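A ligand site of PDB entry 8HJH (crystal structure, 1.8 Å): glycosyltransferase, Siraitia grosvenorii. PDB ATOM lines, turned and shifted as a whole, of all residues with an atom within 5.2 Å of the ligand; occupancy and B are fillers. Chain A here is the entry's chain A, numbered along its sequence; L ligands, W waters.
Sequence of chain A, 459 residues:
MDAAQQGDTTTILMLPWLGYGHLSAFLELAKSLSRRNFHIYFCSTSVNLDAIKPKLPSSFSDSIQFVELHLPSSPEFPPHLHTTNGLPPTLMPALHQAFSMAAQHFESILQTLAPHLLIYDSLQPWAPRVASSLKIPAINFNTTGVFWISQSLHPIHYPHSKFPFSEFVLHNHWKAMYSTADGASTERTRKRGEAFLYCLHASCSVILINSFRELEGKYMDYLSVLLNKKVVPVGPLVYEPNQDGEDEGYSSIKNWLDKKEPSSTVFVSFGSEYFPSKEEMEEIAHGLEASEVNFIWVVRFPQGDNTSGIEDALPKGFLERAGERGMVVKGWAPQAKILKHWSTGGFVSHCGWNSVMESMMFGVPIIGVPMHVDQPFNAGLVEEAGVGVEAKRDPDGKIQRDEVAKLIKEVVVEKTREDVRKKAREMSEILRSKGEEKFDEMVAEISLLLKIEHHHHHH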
ATOM      1  N   TYR A  20     -29.855 -28.528   3.944  1.00  0.00           N
ATOM      2  CA  TYR A  20     -28.637 -29.256   4.269  1.00  0.00           C
ATOM      3  C   TYR A  20     -28.100 -28.907   5.675  1.00  0.00           C
ATOM      4  O   TYR A  20     -27.631 -29.789   6.408  1.00  0.00           O
ATOM      5  CB  TYR A  20     -27.574 -28.976   3.212  1.00  0.00           C
ATOM      6  CG  TYR A  20     -26.304 -29.771   3.451  1.00  0.00           C
ATOM      7  CD1 TYR A  20     -26.152 -31.084   2.957  1.00  0.00           C
ATOM      8  CD2 TYR A  20     -25.262 -29.216   4.178  1.00  0.00           C
ATOM      9  CE1 TYR A  20     -24.957 -31.786   3.197  1.00  0.00           C
ATOM     10  CE2 TYR A  20     -24.079 -29.932   4.422  1.00  0.00           C
ATOM     11  CZ  TYR A  20     -23.942 -31.185   3.953  1.00  0.00           C
ATOM     12  OH  TYR A  20     -22.753 -31.838   4.202  1.00  0.00           O
ATOM     13  N   GLY A  21     -28.164 -27.622   6.049  1.00  0.00           N
ATOM     14  CA  GLY A  21     -27.699 -27.241   7.381  1.00  0.00           C
ATOM     15  C   GLY A  21     -28.523 -27.937   8.443  1.00  0.00           C
ATOM     16  O   GLY A  21     -27.986 -28.319   9.499  1.00  0.00           O
ATOM     17  N   HIS A  22     -29.859 -28.034   8.214  1.00  0.00           N
ATOM     18  CA  HIS A  22     -30.778 -28.673   9.172  1.00  0.00           C
ATOM     19  C   HIS A  22     -30.512 -30.160   9.243  1.00  0.00           C
ATOM     20  O   HIS A  22     -30.391 -30.731  10.346  1.00  0.00           O
ATOM     21  CB  HIS A  22     -32.258 -28.426   8.776  1.00  0.00           C
ATOM     22  CG  HIS A  22     -32.632 -26.972   8.737  1.00  0.00           C
ATOM     23  ND1 HIS A  22     -33.510 -26.429   9.657  1.00  0.00           N
ATOM     24  CD2 HIS A  22     -32.180 -25.930   7.994  1.00  0.00           C
ATOM     25  CE1 HIS A  22     -33.623 -25.131   9.439  1.00  0.00           C
ATOM     26  NE2 HIS A  22     -32.844 -24.805   8.424  1.00  0.00           N
ATOM     27  N   SER A  24     -27.724 -31.611   8.639  1.00  0.00           N
ATOM     28  CA  SER A  24     -26.432 -31.808   9.267  1.00  0.00           C
ATOM     29  C   SER A  24     -26.538 -31.718  10.778  1.00  0.00           C
ATOM     30  O   SER A  24     -25.944 -32.526  11.488  1.00  0.00           O
ATOM     31  CB  SER A  24     -25.415 -30.785   8.757  1.00  0.00           C
ATOM     32  OG  SER A  24     -25.241 -30.826   7.355  1.00  0.00           O
ATOM     33  N   PHE A 267     -11.344 -18.560   4.018  1.00  0.00           N
ATOM     34  CA  PHE A 267     -12.325 -19.383   3.262  1.00  0.00           C
ATOM     35  C   PHE A 267     -13.547 -18.490   3.036  1.00  0.00           C
ATOM     36  O   PHE A 267     -13.953 -17.804   3.977  1.00  0.00           O
ATOM     37  CB  PHE A 267     -12.675 -20.662   4.016  1.00  0.00           C
ATOM     38  CG  PHE A 267     -13.695 -21.529   3.326  1.00  0.00           C
ATOM     39  CD1 PHE A 267     -13.491 -21.976   2.033  1.00  0.00           C
ATOM     40  CD2 PHE A 267     -14.860 -21.905   3.976  1.00  0.00           C
ATOM     41  CE1 PHE A 267     -14.426 -22.779   1.403  1.00  0.00           C
ATOM     42  CE2 PHE A 267     -15.795 -22.708   3.345  1.00  0.00           C
ATOM     43  CZ  PHE A 267     -15.575 -23.142   2.057  1.00  0.00           C
ATOM     44  N   SER A 269     -17.536 -18.415   1.829  1.00  0.00           N
ATOM     45  CA  SER A 269     -18.685 -19.315   1.565  1.00  0.00           C
ATOM     46  C   SER A 269     -19.994 -18.641   1.988  1.00  0.00           C
ATOM     47  O   SER A 269     -20.020 -18.001   3.052  1.00  0.00           O
ATOM     48  CB  SER A 269     -18.529 -20.639   2.256  1.00  0.00           C
ATOM     49  OG  SER A 269     -19.614 -21.498   1.948  1.00  0.00           O
ATOM     50  N   PHE A 270     -21.055 -18.853   1.204  1.00  0.00           N
ATOM     51  CA  PHE A 270     -22.381 -18.259   1.525  1.00  0.00           C
ATOM     52  C   PHE A 270     -23.402 -19.370   1.782  1.00  0.00           C
ATOM     53  O   PHE A 270     -24.613 -19.121   1.632  1.00  0.00           O
ATOM     54  CB  PHE A 270     -22.758 -17.195   0.489  1.00  0.00           C
ATOM     55  CG  PHE A 270     -21.763 -16.066   0.476  1.00  0.00           C
ATOM     56  CD1 PHE A 270     -21.803 -15.095   1.459  1.00  0.00           C
ATOM     57  CD2 PHE A 270     -20.755 -16.022  -0.467  1.00  0.00           C
ATOM     58  CE1 PHE A 270     -20.869 -14.069   1.470  1.00  0.00           C
ATOM     59  CE2 PHE A 270     -19.821 -14.995  -0.455  1.00  0.00           C
ATOM     60  CZ  PHE A 270     -19.878 -14.024   0.524  1.00  0.00           C
ATOM     61  N   GLY A 271     -22.928 -20.569   2.152  1.00  0.00           N
ATOM     62  CA  GLY A 271     -23.854 -21.652   2.526  1.00  0.00           C
ATOM     63  C   GLY A 271     -24.426 -22.439   1.363  1.00  0.00           C
ATOM     64  O   GLY A 271     -23.925 -22.275   0.241  1.00  0.00           O
ATOM     65  N   SER A 272     -25.419 -23.282   1.644  1.00  0.00           N
ATOM     66  CA  SER A 272     -26.012 -24.155   0.601  1.00  0.00           C
ATOM     67  C   SER A 272     -27.326 -23.591   0.054  1.00  0.00           C
ATOM     68  O   SER A 272     -27.860 -24.192  -0.892  1.00  0.00           O
ATOM     69  CB  SER A 272     -26.235 -25.526   1.177  1.00  0.00           C
ATOM     70  OG  SER A 272     -27.129 -25.470   2.271  1.00  0.00           O
ATOM     71  N   GLU A 273     -27.833 -22.500   0.630  1.00  0.00           N
ATOM     72  CA  GLU A 273     -29.177 -21.996   0.220  1.00  0.00           C
ATOM     73  C   GLU A 273     -29.124 -20.592  -0.387  1.00  0.00           C
ATOM     74  O   GLU A 273     -30.209 -20.055  -0.676  1.00  0.00           O
ATOM     75  CB  GLU A 273     -30.111 -21.932   1.420  1.00  0.00           C
ATOM     76  CG  GLU A 273     -30.221 -23.210   2.212  1.00  0.00           C
ATOM     77  CD  GLU A 273     -31.248 -23.113   3.326  1.00  0.00           C
ATOM     78  OE1 GLU A 273     -31.641 -24.164   3.865  1.00  0.00           O
ATOM     79  OE2 GLU A 273     -31.656 -21.984   3.654  1.00  0.00           O
ATOM     80  N   VAL A 298     -15.905 -20.618  -2.657  1.00  0.00           N
ATOM     81  CA  VAL A 298     -16.846 -21.550  -3.280  1.00  0.00           C
ATOM     82  C   VAL A 298     -17.934 -20.734  -3.970  1.00  0.00           C
ATOM     83  O   VAL A 298     -18.643 -19.926  -3.343  1.00  0.00           O
ATOM     84  CB  VAL A 298     -17.420 -22.567  -2.282  1.00  0.00           C
ATOM     85  CG1 VAL A 298     -18.059 -21.907  -1.133  1.00  0.00           C
ATOM     86  CG2 VAL A 298     -18.438 -23.486  -2.958  1.00  0.00           C
ATOM     87  N   GLY A 331     -19.267 -25.037  -6.958  1.00  0.00           N
ATOM     88  CA  GLY A 331     -20.299 -25.876  -6.374  1.00  0.00           C
ATOM     89  C   GLY A 331     -20.241 -26.245  -4.908  1.00  0.00           C
ATOM     90  O   GLY A 331     -21.211 -25.951  -4.212  1.00  0.00           O
ATOM     91  N   TRP A 332     -19.190 -26.910  -4.446  1.00  0.00           N
ATOM     92  CA  TRP A 332     -19.153 -27.389  -3.062  1.00  0.00           C
ATOM     93  C   TRP A 332     -17.706 -27.602  -2.648  1.00  0.00           C
ATOM     94  O   TRP A 332     -16.920 -28.101  -3.455  1.00  0.00           O
ATOM     95  CB  TRP A 332     -19.961 -28.703  -2.958  1.00  0.00           C
ATOM     96  CG  TRP A 332     -20.335 -29.115  -1.572  1.00  0.00           C
ATOM     97  CD1 TRP A 332     -19.768 -30.122  -0.821  1.00  0.00           C
ATOM     98  CD2 TRP A 332     -21.379 -28.564  -0.765  1.00  0.00           C
ATOM     99  NE1 TRP A 332     -20.396 -30.217   0.389  1.00  0.00           N
ATOM    100  CE2 TRP A 332     -21.397 -29.270   0.448  1.00  0.00           C
ATOM    101  CE3 TRP A 332     -22.305 -27.548  -0.971  1.00  0.00           C
ATOM    102  CZ2 TRP A 332     -22.287 -28.977   1.472  1.00  0.00           C
ATOM    103  CZ3 TRP A 332     -23.214 -27.272   0.026  1.00  0.00           C
ATOM    104  CH2 TRP A 332     -23.192 -27.972   1.244  1.00  0.00           C
ATOM    105  N   ALA A 333     -17.370 -27.290  -1.390  1.00  0.00           N
ATOM    106  CA  ALA A 333     -16.022 -27.453  -0.859  1.00  0.00           C
ATOM    107  C   ALA A 333     -16.069 -28.215   0.458  1.00  0.00           C
ATOM    108  O   ALA A 333     -17.089 -28.219   1.148  1.00  0.00           O
ATOM    109  CB  ALA A 333     -15.331 -26.088  -0.641  1.00  0.00           C
ATOM    110  N   PRO A 334     -14.923 -28.873   0.857  1.00  0.00           N
ATOM    111  CA  PRO A 334     -14.854 -29.536   2.170  1.00  0.00           C
ATOM    112  C   PRO A 334     -14.585 -28.454   3.218  1.00  0.00           C
ATOM    113  O   PRO A 334     -13.453 -28.195   3.635  1.00  0.00           O
ATOM    114  CB  PRO A 334     -13.689 -30.529   2.021  1.00  0.00           C
ATOM    115  CG  PRO A 334     -12.816 -29.966   0.931  1.00  0.00           C
ATOM    116  CD  PRO A 334     -13.718 -29.123   0.031  1.00  0.00           C
ATOM    117  N   GLN A 335     -15.667 -27.850   3.674  1.00  0.00           N
ATOM    118  CA  GLN A 335     -15.541 -26.673   4.545  1.00  0.00           C
ATOM    119  C   GLN A 335     -14.784 -26.988   5.832  1.00  0.00           C
ATOM    120  O   GLN A 335     -13.895 -26.217   6.226  1.00  0.00           O
ATOM    121  CB  GLN A 335     -16.925 -26.141   4.850  1.00  0.00           C
ATOM    122  CG  GLN A 335     -16.946 -25.016   5.910  1.00  0.00           C
ATOM    123  CD  GLN A 335     -18.241 -24.175   5.865  1.00  0.00           C
ATOM    124  OE1 GLN A 335     -18.742 -23.822   4.767  1.00  0.00           O
ATOM    125  NE2 GLN A 335     -18.816 -23.889   7.046  1.00  0.00           N
ATOM    126  N   ALA A 336     -15.143 -28.073   6.517  1.00  0.00           N
ATOM    127  CA  ALA A 336     -14.521 -28.359   7.813  1.00  0.00           C
ATOM    128  C   ALA A 336     -13.043 -28.588   7.639  1.00  0.00           C
ATOM    129  O   ALA A 336     -12.221 -28.072   8.403  1.00  0.00           O
ATOM    130  CB  ALA A 336     -15.188 -29.578   8.450  1.00  0.00           C
ATOM    131  N   HIS A 350     -21.433 -16.085   5.335  1.00  0.00           N
ATOM    132  CA  HIS A 350     -22.764 -15.499   5.393  1.00  0.00           C
ATOM    133  C   HIS A 350     -23.349 -15.627   6.788  1.00  0.00           C
ATOM    134  O   HIS A 350     -24.433 -15.107   7.069  1.00  0.00           O
ATOM    135  CB  HIS A 350     -23.709 -16.198   4.395  1.00  0.00           C
ATOM    136  CG  HIS A 350     -24.147 -17.583   4.811  1.00  0.00           C
ATOM    137  ND1 HIS A 350     -23.268 -18.555   5.231  1.00  0.00           N
ATOM    138  CD2 HIS A 350     -25.367 -18.169   4.774  1.00  0.00           C
ATOM    139  CE1 HIS A 350     -23.941 -19.685   5.454  1.00  0.00           C
ATOM    140  NE2 HIS A 350     -25.220 -19.459   5.199  1.00  0.00           N
ATOM    141  N   GLY A 352     -24.257 -18.406   8.469  1.00  0.00           N
ATOM    142  CA  GLY A 352     -25.261 -19.461   8.738  1.00  0.00           C
ATOM    143  C   GLY A 352     -24.875 -20.091  10.058  1.00  0.00           C
ATOM    144  O   GLY A 352     -23.668 -20.150  10.345  1.00  0.00           O
ATOM    145  N   TRP A 353     -25.836 -20.572  10.846  1.00  0.00           N
ATOM    146  CA  TRP A 353     -25.496 -21.037  12.219  1.00  0.00           C
ATOM    147  C   TRP A 353     -24.475 -22.182  12.202  1.00  0.00           C
ATOM    148  O   TRP A 353     -23.553 -22.132  13.036  1.00  0.00           O
ATOM    149  CB  TRP A 353     -26.764 -21.414  12.990  1.00  0.00           C
ATOM    150  CG  TRP A 353     -26.515 -21.570  14.456  1.00  0.00           C
ATOM    151  CD1 TRP A 353     -26.650 -22.706  15.190  1.00  0.00           C
ATOM    152  CD2 TRP A 353     -26.061 -20.551  15.371  1.00  0.00           C
ATOM    153  NE1 TRP A 353     -26.320 -22.471  16.495  1.00  0.00           N
ATOM    154  CE2 TRP A 353     -25.963 -21.157  16.633  1.00  0.00           C
ATOM    155  CE3 TRP A 353     -25.737 -19.196  15.243  1.00  0.00           C
ATOM    156  CZ2 TRP A 353     -25.553 -20.451  17.768  1.00  0.00           C
ATOM    157  CZ3 TRP A 353     -25.335 -18.502  16.357  1.00  0.00           C
ATOM    158  CH2 TRP A 353     -25.245 -19.120  17.600  1.00  0.00           C
ATOM    159  N   ASN A 354     -24.619 -23.157  11.311  1.00  0.00           N
ATOM    160  CA  ASN A 354     -23.681 -24.309  11.351  1.00  0.00           C
ATOM    161  C   ASN A 354     -22.264 -23.794  11.050  1.00  0.00           C
ATOM    162  O   ASN A 354     -21.334 -24.211  11.741  1.00  0.00           O
ATOM    163  CB  ASN A 354     -24.114 -25.456  10.432  1.00  0.00           C
ATOM    164  CG  ASN A 354     -25.407 -26.112  10.880  1.00  0.00           C
ATOM    165  OD1 ASN A 354     -25.389 -26.981  11.748  1.00  0.00           O
ATOM    166  ND2 ASN A 354     -26.519 -25.709  10.300  1.00  0.00           N
ATOM    167  N   SER A 355     -22.141 -22.885  10.082  1.00  0.00           N
ATOM    168  CA  SER A 355     -20.822 -22.312   9.721  1.00  0.00           C
ATOM    169  C   SER A 355     -20.232 -21.550  10.905  1.00  0.00           C
ATOM    170  O   SER A 355     -19.018 -21.695  11.145  1.00  0.00           O
ATOM    171  CB  SER A 355     -20.932 -21.440   8.499  1.00  0.00           C
ATOM    172  OG  SER A 355     -21.235 -22.216   7.352  1.00  0.00           O
ATOM    173  N   VAL A 356     -21.048 -20.774  11.620  1.00  0.00           N
ATOM    174  CA  VAL A 356     -20.575 -20.003  12.801  1.00  0.00           C
ATOM    175  C   VAL A 356     -20.087 -20.975  13.889  1.00  0.00           C
ATOM    176  O   VAL A 356     -19.000 -20.752  14.431  1.00  0.00           O
ATOM    177  CB  VAL A 356     -21.680 -19.074  13.333  1.00  0.00           C
ATOM    178  CG1 VAL A 356     -21.397 -18.567  14.739  1.00  0.00           C
ATOM    179  CG2 VAL A 356     -21.944 -17.910  12.393  1.00  0.00           C
ATOM    180  N   GLU A 358     -19.068 -24.101  13.533  1.00  0.00           N
ATOM    181  CA  GLU A 358     -17.843 -24.796  13.057  1.00  0.00           C
ATOM    182  C   GLU A 358     -16.657 -23.842  13.234  1.00  0.00           C
ATOM    183  O   GLU A 358     -15.632 -24.275  13.771  1.00  0.00           O
ATOM    184  CB  GLU A 358     -17.997 -25.189  11.587  1.00  0.00           C
ATOM    185  CG  GLU A 358     -18.971 -26.325  11.380  1.00  0.00           C
ATOM    186  CD  GLU A 358     -19.572 -26.369   9.988  1.00  0.00           C
ATOM    187  OE1 GLU A 358     -19.098 -25.611   9.121  1.00  0.00           O
ATOM    188  OE2 GLU A 358     -20.497 -27.169   9.771  1.00  0.00           O
ATOM    189  N   GLN A 375     -29.146 -14.747   9.749  1.00  0.00           N
ATOM    190  CA  GLN A 375     -27.737 -14.388   9.606  1.00  0.00           C
ATOM    191  C   GLN A 375     -27.352 -13.044  10.221  1.00  0.00           C
ATOM    192  O   GLN A 375     -26.288 -12.983  10.851  1.00  0.00           O
ATOM    193  CB  GLN A 375     -27.337 -14.498   8.129  1.00  0.00           C
ATOM    194  CG  GLN A 375     -27.524 -15.955   7.655  1.00  0.00           C
ATOM    195  CD  GLN A 375     -27.846 -16.048   6.188  1.00  0.00           C
ATOM    196  OE1 GLN A 375     -27.532 -15.122   5.414  1.00  0.00           O
ATOM    197  NE2 GLN A 375     -28.493 -17.159   5.776  1.00  0.00           N
HETATM  198  N1  LIG L   1     -20.920 -26.551   3.591  1.00  0.00           N
HETATM  199  C1  LIG L   1     -19.924 -27.334   3.039  1.00  0.00           C
HETATM  200  N2  LIG L   1     -19.427 -26.903   1.832  1.00  0.00           N
HETATM  201  C2  LIG L   1     -19.789 -25.772   1.162  1.00  0.00           C
HETATM  202  C3  LIG L   1     -20.774 -24.959   1.812  1.00  0.00           C
HETATM  203  C4  LIG L   1     -21.296 -25.374   2.999  1.00  0.00           C
HETATM  204  O1  LIG L   1     -19.592 -28.376   3.580  1.00  0.00           O
HETATM  205  O2  LIG L   1     -19.228 -25.459   0.088  1.00  0.00           O
HETATM  206  C5  LIG L   1     -21.553 -26.982   4.858  1.00  0.00           C
HETATM  207  C6  LIG L   1     -21.111 -26.131   6.085  1.00  0.00           C
HETATM  208  O3  LIG L   1     -19.963 -26.723   6.691  1.00  0.00           O
HETATM  209  C7  LIG L   1     -22.319 -26.269   6.983  1.00  0.00           C
HETATM  210  C8  LIG L   1     -23.499 -26.319   5.999  1.00  0.00           C
HETATM  211  O4  LIG L   1     -22.940 -26.637   4.688  1.00  0.00           O
HETATM  212  O5  LIG L   1     -22.286 -27.456   7.780  1.00  0.00           O
HETATM  213  C9  LIG L   1     -24.099 -24.953   5.893  1.00  0.00           C
HETATM  214  O6  LIG L   1     -24.918 -24.738   7.019  1.00  0.00           O
HETATM  215  P1  LIG L   1     -25.205 -23.224   7.510  1.00  0.00           P
HETATM  216  O7  LIG L   1     -23.895 -22.538   7.763  1.00  0.00           O
HETATM  217  O8  LIG L   1     -26.138 -23.408   8.699  1.00  0.00           O
HETATM  218  O9  LIG L   1     -25.862 -22.355   6.341  1.00  0.00           O
HETATM  219  P2  LIG L   1     -27.067 -22.692   5.263  1.00  0.00           P
HETATM  220  O10 LIG L   1     -27.456 -21.314   4.880  1.00  0.00           O
HETATM  221  O11 LIG L   1     -28.180 -23.384   6.035  1.00  0.00           O
HETATM  222  O12 LIG L   1     -26.491 -23.512   4.131  1.00  0.00           O
HETATM  223  O   HOH W   1     -22.099 -30.262   7.854  1.00  0.00           O
HETATM  224  O   HOH W   2     -18.508 -30.760   2.997  1.00  0.00           O
HETATM  225  O   HOH W   3     -19.309 -29.265   7.233  1.00  0.00           O
HETATM  226  O   HOH W   4     -29.751 -25.339   5.300  1.00  0.00           O
HETATM  227  O   HOH W   5     -28.857 -22.957   9.260  1.00  0.00           O
HETATM  228  O   HOH W   6     -27.099 -20.286   2.438  1.00  0.00           O
HETATM  229  O   HOH W   7     -20.847 -22.268   4.215  1.00  0.00           O
HETATM  230  O   HOH W   8     -31.036 -22.354   7.305  1.00  0.00           O
HETATM  231  O   HOH W   9     -29.895 -20.299   5.206  1.00  0.00           O
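The side-chain carboxylate (OE2) of Glu 358 sits at hydrogen-bond distance from an oxygen (O5) of the ligand (2.7 Å).
The backbone NH (N) of Ser 355 sits at hydrogen-bond distance from an oxygen (O7) of the ligand (2.9 Å).
An oxygen (O7) of the ligand sits at hydrogen-bond distance from the side-chain hydroxyl (OG) of Ser 355 (2.7 Å).
The backbone NH of Ser 272 sits at hydrogen-bond distance from an oxygen (O12) of the ligand (2.7 Å).
An oxygen (O12) of the ligand sits at hydrogen-bond distance from the side-chain hydroxyl (OG) of Ser 272 (2.8 Å).
N of Ala 333 lies within hydrogen-bond range of O2 of the ligand, at 3.0 Å.
The backbone carbonyl oxygen of Ala 333 lies within hydrogen-bond range of a nitrogen (N2) of the ligand.
The backbone NH (N) of Asn 354 is in hydrogen-bond range of an oxygen (O8) of the ligand.
An oxygen (O8) of the ligand lies within hydrogen-bond range of the side-chain amide nitrogen of Asn 354, 2.8 Å away.
A ring nitrogen (NE2) of His 350 sits at hydrogen-bond distance from an oxygen (O10) of the ligand (2.9 Å).
NE2 of Gln 335 sits at hydrogen-bond distance from O3 of the ligand (3.1 Å).
OE1 of Glu 358 is in hydrogen-bond range of NE2 of Gln 335, 2.7 Å away.
OG of Ser 355 sits at hydrogen-bond distance from NE2 of Gln 335 (3.0 Å).
The side-chain amide nitrogen (ND2) of Asn 354 sits at hydrogen-bond distance from the backbone carbonyl oxygen (O) of Gly 21, 3.1 Å away.
A ring nitrogen (ND1) of His 350 lies close to the backbone NH (N) of Gly 352, 3.4 Å away.
N of His 350 lies within hydrogen-bond range of O of Ser 269.
The side-chain hydroxyl (OG) of Ser 24 is in hydrogen-bond range of the backbone carbonyl oxygen (O) of Tyr 20, 2.8 Å away.
N of Gly 271 sits at hydrogen-bond distance from OG of Ser 269, at 3.4 Å.
CE2 of Tyr 20 touches O4 of the ligand, at 3.5 Å.
CA of Gly 21 touches O6 of the ligand, at 3.8 Å.
OG of Ser 269 touches C3 of the ligand, 3.7 Å away.
Gly 271 touches the ligand.
N of Glu 273 touches O12 of the ligand, at 3.9 Å.
CG2 of Val 298 touches O2 of the ligand, at 3.7 Å.
CZ2 of Trp 332 touches C1 of the ligand, at 3.3 Å.
Gly 352 touches the ligand.
Trp 353 touches the ligand.
Hydrophobic or aromatic side chains within 4 Å of the ligand: Tyr 20, Val 298, Trp 332 and His 350.
Of the 25 residues printed, 16 come within 4 Å of the ligand.
Water W4 lies within hydrogen-bond range of an oxygen (O11) of the ligand (2.6 Å), the side-chain carboxylate of Glu 273 (2.6 Å), the backbone NH of Gly 21 (2.9 Å) and the backbone NH of Tyr 20 (3.5 Å).
Water W9 lies within hydrogen-bond range of O10 of the ligand, OE2 of Glu 273 and NE2 of Gln 375.
Water W6 lies within hydrogen-bond range of an oxygen (O10) of the ligand (2.7 Å), the backbone carbonyl oxygen (O) of Phe 270 (2.9 Å), the backbone NH (N) of Glu 273 (3.0 Å) and a ring nitrogen (NE2) of His 350 (3.4 Å).
Water W2 lies within hydrogen-bond range of O1 of the ligand (2.7 Å), NE1 of Trp 332 (3.3 Å) and O of Ala 333 (3.4 Å).
Water W8 bridges a ring nitrogen (NE2) of His 22 (3.2 Å) and an oxygen (O11) of the ligand (3.3 Å).
Water W7 lies within hydrogen-bond range of OE1 of Gln 335 (2.7 Å), OG of Ser 269 (2.7 Å), OG of Ser 355 (3.2 Å) and N of Gly 271 (3.4 Å).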
